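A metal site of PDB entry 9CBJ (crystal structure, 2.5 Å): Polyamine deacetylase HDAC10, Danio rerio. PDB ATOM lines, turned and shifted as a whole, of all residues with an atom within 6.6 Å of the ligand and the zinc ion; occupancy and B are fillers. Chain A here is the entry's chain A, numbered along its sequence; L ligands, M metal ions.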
ATOM      1  N   GLU A  24     -20.459  27.471 -13.470  1.00  0.00           N
ATOM      2  CA  GLU A  24     -19.419  27.862 -14.412  1.00  0.00           C
ATOM      3  C   GLU A  24     -18.560  26.688 -14.829  1.00  0.00           C
ATOM      4  O   GLU A  24     -18.114  26.616 -15.987  1.00  0.00           O
ATOM      5  CB  GLU A  24     -18.565  28.956 -13.781  1.00  0.00           C
ATOM      6  CG  GLU A  24     -17.849  29.861 -14.750  1.00  0.00           C
ATOM      7  CD  GLU A  24     -17.168  31.017 -14.048  1.00  0.00           C
ATOM      8  OE1 GLU A  24     -16.673  30.812 -12.920  1.00  0.00           O
ATOM      9  OE2 GLU A  24     -17.155  32.131 -14.621  1.00  0.00           O
ATOM     10  N   CYS A  25     -18.330  25.738 -13.919  1.00  0.00           N
ATOM     11  CA  CYS A  25     -17.421  24.626 -14.159  1.00  0.00           C
ATOM     12  C   CYS A  25     -18.125  23.281 -14.319  1.00  0.00           C
ATOM     13  O   CYS A  25     -17.451  22.277 -14.526  1.00  0.00           O
ATOM     14  CB  CYS A  25     -16.393  24.525 -13.031  1.00  0.00           C
ATOM     15  SG  CYS A  25     -15.363  25.982 -12.813  1.00  0.00           S
ATOM     16  N   ILE A  27     -19.471  21.838 -16.595  1.00  0.00           N
ATOM     17  CA  ILE A  27     -19.294  21.161 -17.873  1.00  0.00           C
ATOM     18  C   ILE A  27     -18.008  20.330 -17.907  1.00  0.00           C
ATOM     19  O   ILE A  27     -17.934  19.329 -18.622  1.00  0.00           O
ATOM     20  CB  ILE A  27     -19.319  22.170 -19.020  1.00  0.00           C
ATOM     21  CG1 ILE A  27     -18.356  23.325 -18.730  1.00  0.00           C
ATOM     22  CG2 ILE A  27     -20.736  22.676 -19.258  1.00  0.00           C
ATOM     23  CD1 ILE A  27     -18.172  24.279 -19.881  1.00  0.00           C
ATOM     24  N   ASN A  93     -10.140  32.510 -11.693  1.00  0.00           N
ATOM     25  CA  ASN A  93     -11.348  32.679 -12.496  1.00  0.00           C
ATOM     26  C   ASN A  93     -11.688  31.384 -13.229  1.00  0.00           C
ATOM     27  O   ASN A  93     -10.838  30.843 -13.952  1.00  0.00           O
ATOM     28  CB  ASN A  93     -11.191  33.823 -13.490  1.00  0.00           C
ATOM     29  CG  ASN A  93     -12.417  34.025 -14.354  1.00  0.00           C
ATOM     30  OD1 ASN A  93     -12.322  34.165 -15.572  1.00  0.00           O
ATOM     31  ND2 ASN A  93     -13.582  34.029 -13.725  1.00  0.00           N
ATOM     32  N   ALA A  94     -12.917  30.904 -13.041  1.00  0.00           N
ATOM     33  CA  ALA A  94     -13.447  29.737 -13.755  1.00  0.00           C
ATOM     34  C   ALA A  94     -12.574  28.508 -13.528  1.00  0.00           C
ATOM     35  O   ALA A  94     -12.163  27.828 -14.472  1.00  0.00           O
ATOM     36  CB  ALA A  94     -13.619  30.033 -15.248  1.00  0.00           C
ATOM     37  N   PRO A 134      -7.143  20.635 -19.094  1.00  0.00           N
ATOM     38  CA  PRO A 134      -6.581  21.369 -20.239  1.00  0.00           C
ATOM     39  C   PRO A 134      -5.558  22.389 -19.778  1.00  0.00           C
ATOM     40  O   PRO A 134      -5.340  22.556 -18.583  1.00  0.00           O
ATOM     41  CB  PRO A 134      -7.808  22.028 -20.876  1.00  0.00           C
ATOM     42  CG  PRO A 134      -8.781  22.158 -19.755  1.00  0.00           C
ATOM     43  CD  PRO A 134      -8.572  20.945 -18.892  1.00  0.00           C
ATOM     44  N   HIS A 136      -4.456  25.632 -22.009  1.00  0.00           N
ATOM     45  CA  HIS A 136      -4.119  26.832 -22.772  1.00  0.00           C
ATOM     46  C   HIS A 136      -4.556  28.140 -22.112  1.00  0.00           C
ATOM     47  O   HIS A 136      -4.165  29.206 -22.589  1.00  0.00           O
ATOM     48  CB  HIS A 136      -4.690  26.733 -24.195  1.00  0.00           C
ATOM     49  CG  HIS A 136      -6.183  26.801 -24.274  1.00  0.00           C
ATOM     50  ND1 HIS A 136      -6.843  27.333 -25.366  1.00  0.00           N
ATOM     51  CD2 HIS A 136      -7.151  26.395 -23.416  1.00  0.00           C
ATOM     52  CE1 HIS A 136      -8.154  27.245 -25.172  1.00  0.00           C
ATOM     53  NE2 HIS A 136      -8.365  26.684 -23.998  1.00  0.00           N
ATOM     54  N   HIS A 137      -5.328  28.092 -21.025  1.00  0.00           N
ATOM     55  CA  HIS A 137      -5.693  29.312 -20.312  1.00  0.00           C
ATOM     56  C   HIS A 137      -4.809  29.583 -19.102  1.00  0.00           C
ATOM     57  O   HIS A 137      -4.827  30.707 -18.579  1.00  0.00           O
ATOM     58  CB  HIS A 137      -7.153  29.254 -19.851  1.00  0.00           C
ATOM     59  CG  HIS A 137      -8.141  29.265 -20.971  1.00  0.00           C
ATOM     60  ND1 HIS A 137      -8.255  30.322 -21.862  1.00  0.00           N
ATOM     61  CD2 HIS A 137      -9.077  28.363 -21.340  1.00  0.00           C
ATOM     62  CE1 HIS A 137      -9.205  30.055 -22.737  1.00  0.00           C
ATOM     63  NE2 HIS A 137      -9.730  28.873 -22.443  1.00  0.00           N
ATOM     64  N   ASN A 144      -6.511  29.185 -14.545  1.00  0.00           N
ATOM     65  CA  ASN A 144      -7.534  29.968 -15.236  1.00  0.00           C
ATOM     66  C   ASN A 144      -8.271  29.071 -16.213  1.00  0.00           C
ATOM     67  O   ASN A 144      -7.659  28.264 -16.908  1.00  0.00           O
ATOM     68  CB  ASN A 144      -6.908  31.159 -15.973  1.00  0.00           C
ATOM     69  CG  ASN A 144      -7.941  32.136 -16.466  1.00  0.00           C
ATOM     70  OD1 ASN A 144      -8.407  32.050 -17.599  1.00  0.00           O
ATOM     71  ND2 ASN A 144      -8.321  33.085 -15.613  1.00  0.00           N
ATOM     72  N   GLY A 145      -9.597  29.217 -16.247  1.00  0.00           N
ATOM     73  CA  GLY A 145     -10.435  28.532 -17.222  1.00  0.00           C
ATOM     74  C   GLY A 145     -10.202  27.032 -17.336  1.00  0.00           C
ATOM     75  O   GLY A 145      -9.815  26.547 -18.398  1.00  0.00           O
ATOM     76  N   PHE A 146     -10.434  26.315 -16.238  1.00  0.00           N
ATOM     77  CA  PHE A 146     -10.292  24.858 -16.137  1.00  0.00           C
ATOM     78  C   PHE A 146      -8.852  24.381 -16.271  1.00  0.00           C
ATOM     79  O   PHE A 146      -8.612  23.171 -16.306  1.00  0.00           O
ATOM     80  CB  PHE A 146     -11.138  24.101 -17.173  1.00  0.00           C
ATOM     81  CG  PHE A 146     -12.591  24.514 -17.241  1.00  0.00           C
ATOM     82  CD1 PHE A 146     -13.198  25.194 -16.196  1.00  0.00           C
ATOM     83  CD2 PHE A 146     -13.352  24.214 -18.361  1.00  0.00           C
ATOM     84  CE1 PHE A 146     -14.523  25.585 -16.278  1.00  0.00           C
ATOM     85  CE2 PHE A 146     -14.678  24.588 -18.448  1.00  0.00           C
ATOM     86  CZ  PHE A 146     -15.270  25.275 -17.407  1.00  0.00           C
ATOM     87  N   CYS A 147      -7.880  25.294 -16.339  1.00  0.00           N
ATOM     88  CA  CYS A 147      -6.501  24.945 -16.637  1.00  0.00           C
ATOM     89  C   CYS A 147      -5.614  25.231 -15.439  1.00  0.00           C
ATOM     90  O   CYS A 147      -5.687  26.305 -14.845  1.00  0.00           O
ATOM     91  CB  CYS A 147      -5.998  25.723 -17.855  1.00  0.00           C
ATOM     92  SG  CYS A 147      -6.938  25.405 -19.371  1.00  0.00           S
ATOM     93  N   ASP A 174      -9.319  25.462 -30.291  1.00  0.00           N
ATOM     94  CA  ASP A 174     -10.340  25.568 -29.261  1.00  0.00           C
ATOM     95  C   ASP A 174     -11.154  26.833 -29.477  1.00  0.00           C
ATOM     96  O   ASP A 174     -10.681  27.816 -30.057  1.00  0.00           O
ATOM     97  CB  ASP A 174      -9.690  25.558 -27.876  1.00  0.00           C
ATOM     98  CG  ASP A 174     -10.699  25.409 -26.745  1.00  0.00           C
ATOM     99  OD1 ASP A 174     -11.502  26.340 -26.531  1.00  0.00           O
ATOM    100  OD2 ASP A 174     -10.674  24.369 -26.068  1.00  0.00           O
ATOM    101  N   VAL A 175     -12.410  26.810 -29.019  1.00  0.00           N
ATOM    102  CA  VAL A 175     -13.292  27.950 -29.248  1.00  0.00           C
ATOM    103  C   VAL A 175     -12.963  29.118 -28.335  1.00  0.00           C
ATOM    104  O   VAL A 175     -13.407  30.248 -28.586  1.00  0.00           O
ATOM    105  CB  VAL A 175     -14.766  27.545 -29.091  1.00  0.00           C
ATOM    106  CG1 VAL A 175     -15.181  27.568 -27.625  1.00  0.00           C
ATOM    107  CG2 VAL A 175     -15.667  28.444 -29.932  1.00  0.00           C
ATOM    108  N   HIS A 176     -12.183  28.892 -27.280  1.00  0.00           N
ATOM    109  CA  HIS A 176     -11.745  29.966 -26.397  1.00  0.00           C
ATOM    110  C   HIS A 176     -10.331  30.394 -26.754  1.00  0.00           C
ATOM    111  O   HIS A 176      -9.554  29.632 -27.352  1.00  0.00           O
ATOM    112  CB  HIS A 176     -11.813  29.529 -24.929  1.00  0.00           C
ATOM    113  CG  HIS A 176     -13.189  29.174 -24.467  1.00  0.00           C
ATOM    114  ND1 HIS A 176     -13.729  27.911 -24.613  1.00  0.00           N
ATOM    115  CD2 HIS A 176     -14.135  29.918 -23.851  1.00  0.00           C
ATOM    116  CE1 HIS A 176     -14.952  27.899 -24.117  1.00  0.00           C
ATOM    117  NE2 HIS A 176     -15.227  29.105 -23.649  1.00  0.00           N
ATOM    118  N   HIS A 177      -9.992  31.622 -26.390  1.00  0.00           N
ATOM    119  CA  HIS A 177      -8.678  32.174 -26.694  1.00  0.00           C
ATOM    120  C   HIS A 177      -7.678  31.703 -25.655  1.00  0.00           C
ATOM    121  O   HIS A 177      -7.783  32.060 -24.475  1.00  0.00           O
ATOM    122  CB  HIS A 177      -8.720  33.688 -26.746  1.00  0.00           C
ATOM    123  CG  HIS A 177      -7.386  34.319 -26.977  1.00  0.00           C
ATOM    124  ND1 HIS A 177      -6.848  35.277 -26.136  1.00  0.00           N
ATOM    125  CD2 HIS A 177      -6.448  34.105 -27.934  1.00  0.00           C
ATOM    126  CE1 HIS A 177      -5.668  35.633 -26.578  1.00  0.00           C
ATOM    127  NE2 HIS A 177      -5.392  34.941 -27.670  1.00  0.00           N
ATOM    128  N   PHE A 204     -17.365  37.956 -24.923  1.00  0.00           N
ATOM    129  CA  PHE A 204     -17.277  36.548 -24.557  1.00  0.00           C
ATOM    130  C   PHE A 204     -16.015  36.287 -23.744  1.00  0.00           C
ATOM    131  O   PHE A 204     -14.978  36.930 -23.931  1.00  0.00           O
ATOM    132  CB  PHE A 204     -17.298  35.655 -25.799  1.00  0.00           C
ATOM    133  CG  PHE A 204     -17.439  34.196 -25.473  1.00  0.00           C
ATOM    134  CD1 PHE A 204     -18.645  33.692 -24.997  1.00  0.00           C
ATOM    135  CD2 PHE A 204     -16.382  33.325 -25.663  1.00  0.00           C
ATOM    136  CE1 PHE A 204     -18.778  32.350 -24.699  1.00  0.00           C
ATOM    137  CE2 PHE A 204     -16.516  31.983 -25.365  1.00  0.00           C
ATOM    138  CZ  PHE A 204     -17.713  31.491 -24.889  1.00  0.00           C
ATOM    139  N   TRP A 205     -16.109  35.318 -22.839  1.00  0.00           N
ATOM    140  CA  TRP A 205     -15.005  34.994 -21.947  1.00  0.00           C
ATOM    141  C   TRP A 205     -13.784  34.563 -22.752  1.00  0.00           C
ATOM    142  O   TRP A 205     -13.920  33.815 -23.735  1.00  0.00           O
ATOM    143  CB  TRP A 205     -15.433  33.890 -20.983  1.00  0.00           C
ATOM    144  CG  TRP A 205     -14.488  33.674 -19.858  1.00  0.00           C
ATOM    145  CD1 TRP A 205     -14.578  34.201 -18.604  1.00  0.00           C
ATOM    146  CD2 TRP A 205     -13.307  32.883 -19.882  1.00  0.00           C
ATOM    147  NE1 TRP A 205     -13.512  33.786 -17.839  1.00  0.00           N
ATOM    148  CE2 TRP A 205     -12.712  32.977 -18.607  1.00  0.00           C
ATOM    149  CE3 TRP A 205     -12.666  32.108 -20.861  1.00  0.00           C
ATOM    150  CZ2 TRP A 205     -11.529  32.315 -18.283  1.00  0.00           C
ATOM    151  CZ3 TRP A 205     -11.502  31.460 -20.539  1.00  0.00           C
ATOM    152  CH2 TRP A 205     -10.936  31.565 -19.256  1.00  0.00           C
ATOM    153  N   GLY A 265      -9.015  21.754 -29.012  1.00  0.00           N
ATOM    154  CA  GLY A 265     -10.218  21.955 -28.251  1.00  0.00           C
ATOM    155  C   GLY A 265     -11.410  21.811 -29.158  1.00  0.00           C
ATOM    156  O   GLY A 265     -11.553  22.543 -30.147  1.00  0.00           O
ATOM    157  N   ASP A 267     -14.612  22.153 -28.307  1.00  0.00           N
ATOM    158  CA  ASP A 267     -15.771  22.989 -28.004  1.00  0.00           C
ATOM    159  C   ASP A 267     -16.081  23.968 -29.128  1.00  0.00           C
ATOM    160  O   ASP A 267     -16.988  24.792 -28.977  1.00  0.00           O
ATOM    161  CB  ASP A 267     -15.552  23.737 -26.686  1.00  0.00           C
ATOM    162  CG  ASP A 267     -14.202  24.427 -26.622  1.00  0.00           C
ATOM    163  OD1 ASP A 267     -13.456  24.395 -27.621  1.00  0.00           O
ATOM    164  OD2 ASP A 267     -13.899  25.007 -25.566  1.00  0.00           O
ATOM    165  N   GLU A 274     -20.716  25.672 -25.030  1.00  0.00           N
ATOM    166  CA  GLU A 274     -19.858  26.817 -24.762  1.00  0.00           C
ATOM    167  C   GLU A 274     -19.528  27.607 -26.023  1.00  0.00           C
ATOM    168  O   GLU A 274     -19.501  28.842 -25.989  1.00  0.00           O
ATOM    169  CB  GLU A 274     -18.566  26.362 -24.076  1.00  0.00           C
ATOM    170  CG  GLU A 274     -18.141  27.218 -22.899  1.00  0.00           C
ATOM    171  CD  GLU A 274     -19.093  27.114 -21.729  1.00  0.00           C
ATOM    172  OE1 GLU A 274     -19.927  26.180 -21.702  1.00  0.00           O
ATOM    173  OE2 GLU A 274     -19.022  27.980 -20.823  1.00  0.00           O
ATOM    174  N   GLU A 304      -7.804  19.925 -25.363  1.00  0.00           N
ATOM    175  CA  GLU A 304      -8.112  21.074 -24.530  1.00  0.00           C
ATOM    176  C   GLU A 304      -9.577  21.003 -24.104  1.00  0.00           C
ATOM    177  O   GLU A 304      -9.920  20.215 -23.223  1.00  0.00           O
ATOM    178  CB  GLU A 304      -7.838  22.388 -25.276  1.00  0.00           C
ATOM    179  CG  GLU A 304      -6.395  22.547 -25.744  1.00  0.00           C
ATOM    180  CD  GLU A 304      -5.481  23.105 -24.667  1.00  0.00           C
ATOM    181  OE1 GLU A 304      -5.986  23.492 -23.596  1.00  0.00           O
ATOM    182  OE2 GLU A 304      -4.254  23.159 -24.909  1.00  0.00           O
ATOM    183  N   GLY A 305     -10.441  21.784 -24.743  1.00  0.00           N
ATOM    184  CA  GLY A 305     -11.847  21.838 -24.404  1.00  0.00           C
ATOM    185  C   GLY A 305     -12.665  20.818 -25.162  1.00  0.00           C
ATOM    186  O   GLY A 305     -12.137  19.887 -25.790  1.00  0.00           O
ATOM    187  N   GLY A 306     -13.987  21.004 -25.128  1.00  0.00           N
ATOM    188  CA  GLY A 306     -14.919  20.080 -25.741  1.00  0.00           C
ATOM    189  C   GLY A 306     -15.811  19.430 -24.700  1.00  0.00           C
ATOM    190  O   GLY A 306     -15.340  18.614 -23.904  1.00  0.00           O
ATOM    191  N   TYR A 307     -17.107  19.755 -24.711  1.00  0.00           N
ATOM    192  CA  TYR A 307     -17.970  19.421 -23.584  1.00  0.00           C
ATOM    193  C   TYR A 307     -19.276  18.743 -23.953  1.00  0.00           C
ATOM    194  O   TYR A 307     -19.965  18.255 -23.050  1.00  0.00           O
ATOM    195  CB  TYR A 307     -18.257  20.688 -22.761  1.00  0.00           C
ATOM    196  CG  TYR A 307     -16.958  21.379 -22.376  1.00  0.00           C
ATOM    197  CD1 TYR A 307     -16.197  20.905 -21.316  1.00  0.00           C
ATOM    198  CD2 TYR A 307     -16.475  22.454 -23.099  1.00  0.00           C
ATOM    199  CE1 TYR A 307     -15.002  21.508 -20.973  1.00  0.00           C
ATOM    200  CE2 TYR A 307     -15.286  23.070 -22.757  1.00  0.00           C
ATOM    201  CZ  TYR A 307     -14.553  22.591 -21.694  1.00  0.00           C
ATOM    202  OH  TYR A 307     -13.360  23.185 -21.345  1.00  0.00           O
HETATM  203  C1  LIG L   1     -11.870  26.258 -21.223  1.00  0.00           C
HETATM  204  C2  LIG L   1     -13.373  26.491 -21.322  1.00  0.00           C
HETATM  205  C3  LIG L   1     -14.110  27.469 -20.451  1.00  0.00           C
HETATM  206  C4  LIG L   1     -15.494  27.444 -20.309  1.00  0.00           C
HETATM  207  C5  LIG L   1     -16.180  28.370 -19.494  1.00  0.00           C
HETATM  208  C6  LIG L   1     -15.538  29.386 -18.767  1.00  0.00           C
HETATM  209  C7  LIG L   1     -16.300  30.392 -17.900  1.00  0.00           C
HETATM  210  C8  LIG L   1     -16.945  31.593 -18.653  1.00  0.00           C
HETATM  211  C9  LIG L   1     -18.433  31.960 -18.327  1.00  0.00           C
HETATM  212  C10 LIG L   1     -14.123  29.408 -18.923  1.00  0.00           C
HETATM  213  C11 LIG L   1     -13.422  28.489 -19.742  1.00  0.00           C
HETATM  214  N1  LIG L   1     -18.664  32.209 -16.888  1.00  0.00           N
HETATM  215  O1  LIG L   1     -14.007  25.829 -22.183  1.00  0.00           O
HETATM  216  S1  LIG L   1     -11.197  25.414 -22.729  1.00  0.00           S
HETATM  217 ZN    ZN M   1     -12.444  26.008 -24.645  1.00  0.00          ZN
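OD1 of Asp 267 is in hydrogen-bond range of N of Val 175. A ring nitrogen (NE2) of His 137 lies within hydrogen-bond range of a ring nitrogen (NE2) of His 136 (3.0 Å). The side-chain carboxylate of Glu 304 sits at hydrogen-bond distance from the backbone NH of His 136. The side-chain sulfur of Cys 147 lies within hydrogen-bond range of the backbone NH of His 137 (3.5 Å). O of His 177 sits close to ND1 of His 137 (3.2 Å). The backbone carbonyl oxygen (O) of Gly 145 is in hydrogen-bond range of the side-chain sulfur (SG) of Cys 147 (3.2 Å). The backbone NH (N) of Gly 145 sits at hydrogen-bond distance from the backbone carbonyl oxygen (O) of Asn 93. The backbone NH of Phe 146 is in hydrogen-bond range of the backbone carbonyl oxygen of Ala 94 (2.9 Å).
Residues that only touch the ligand: Ala 94 (3.8 Å), Gly 145 (3.5 Å), Phe 146 (3.5 Å), Trp 205 (3.4 Å) and Glu 274 (3.2 Å). Hydrophobic or aromatic side chains that line the ligand: Ala 94, His 137, Phe 146, His 176, Trp 205 and Tyr 307.
The zinc ion is bound by the side-chain carboxylate (OD2) of Asp 267 (2.0 Å), the side-chain carboxylate (OD1) of Asp 174 (2.1 Å), a ring nitrogen (ND1) of His 176 (2.3 Å) and a sulfur (S1) of the ligand (2.4 Å). The zinc ion has four donor atoms within binding distance. Slightly farther from the zinc ion lies the side-chain carboxylate (OD2) of Asp 174 (2.8 Å).
OE2 of Glu 24 lies within salt-bridge range of N1 of the ligand (2.7 Å). The side-chain hydroxyl (OH) of Tyr 307 lies within hydrogen-bond range of an oxygen (O1) of the ligand, at 2.8 Å. A sulfur (S1) of the ligand sits close to a ring nitrogen (NE2) of His 136 (3.4 Å). NE2 of His 137 sits close to S1 of the ligand.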
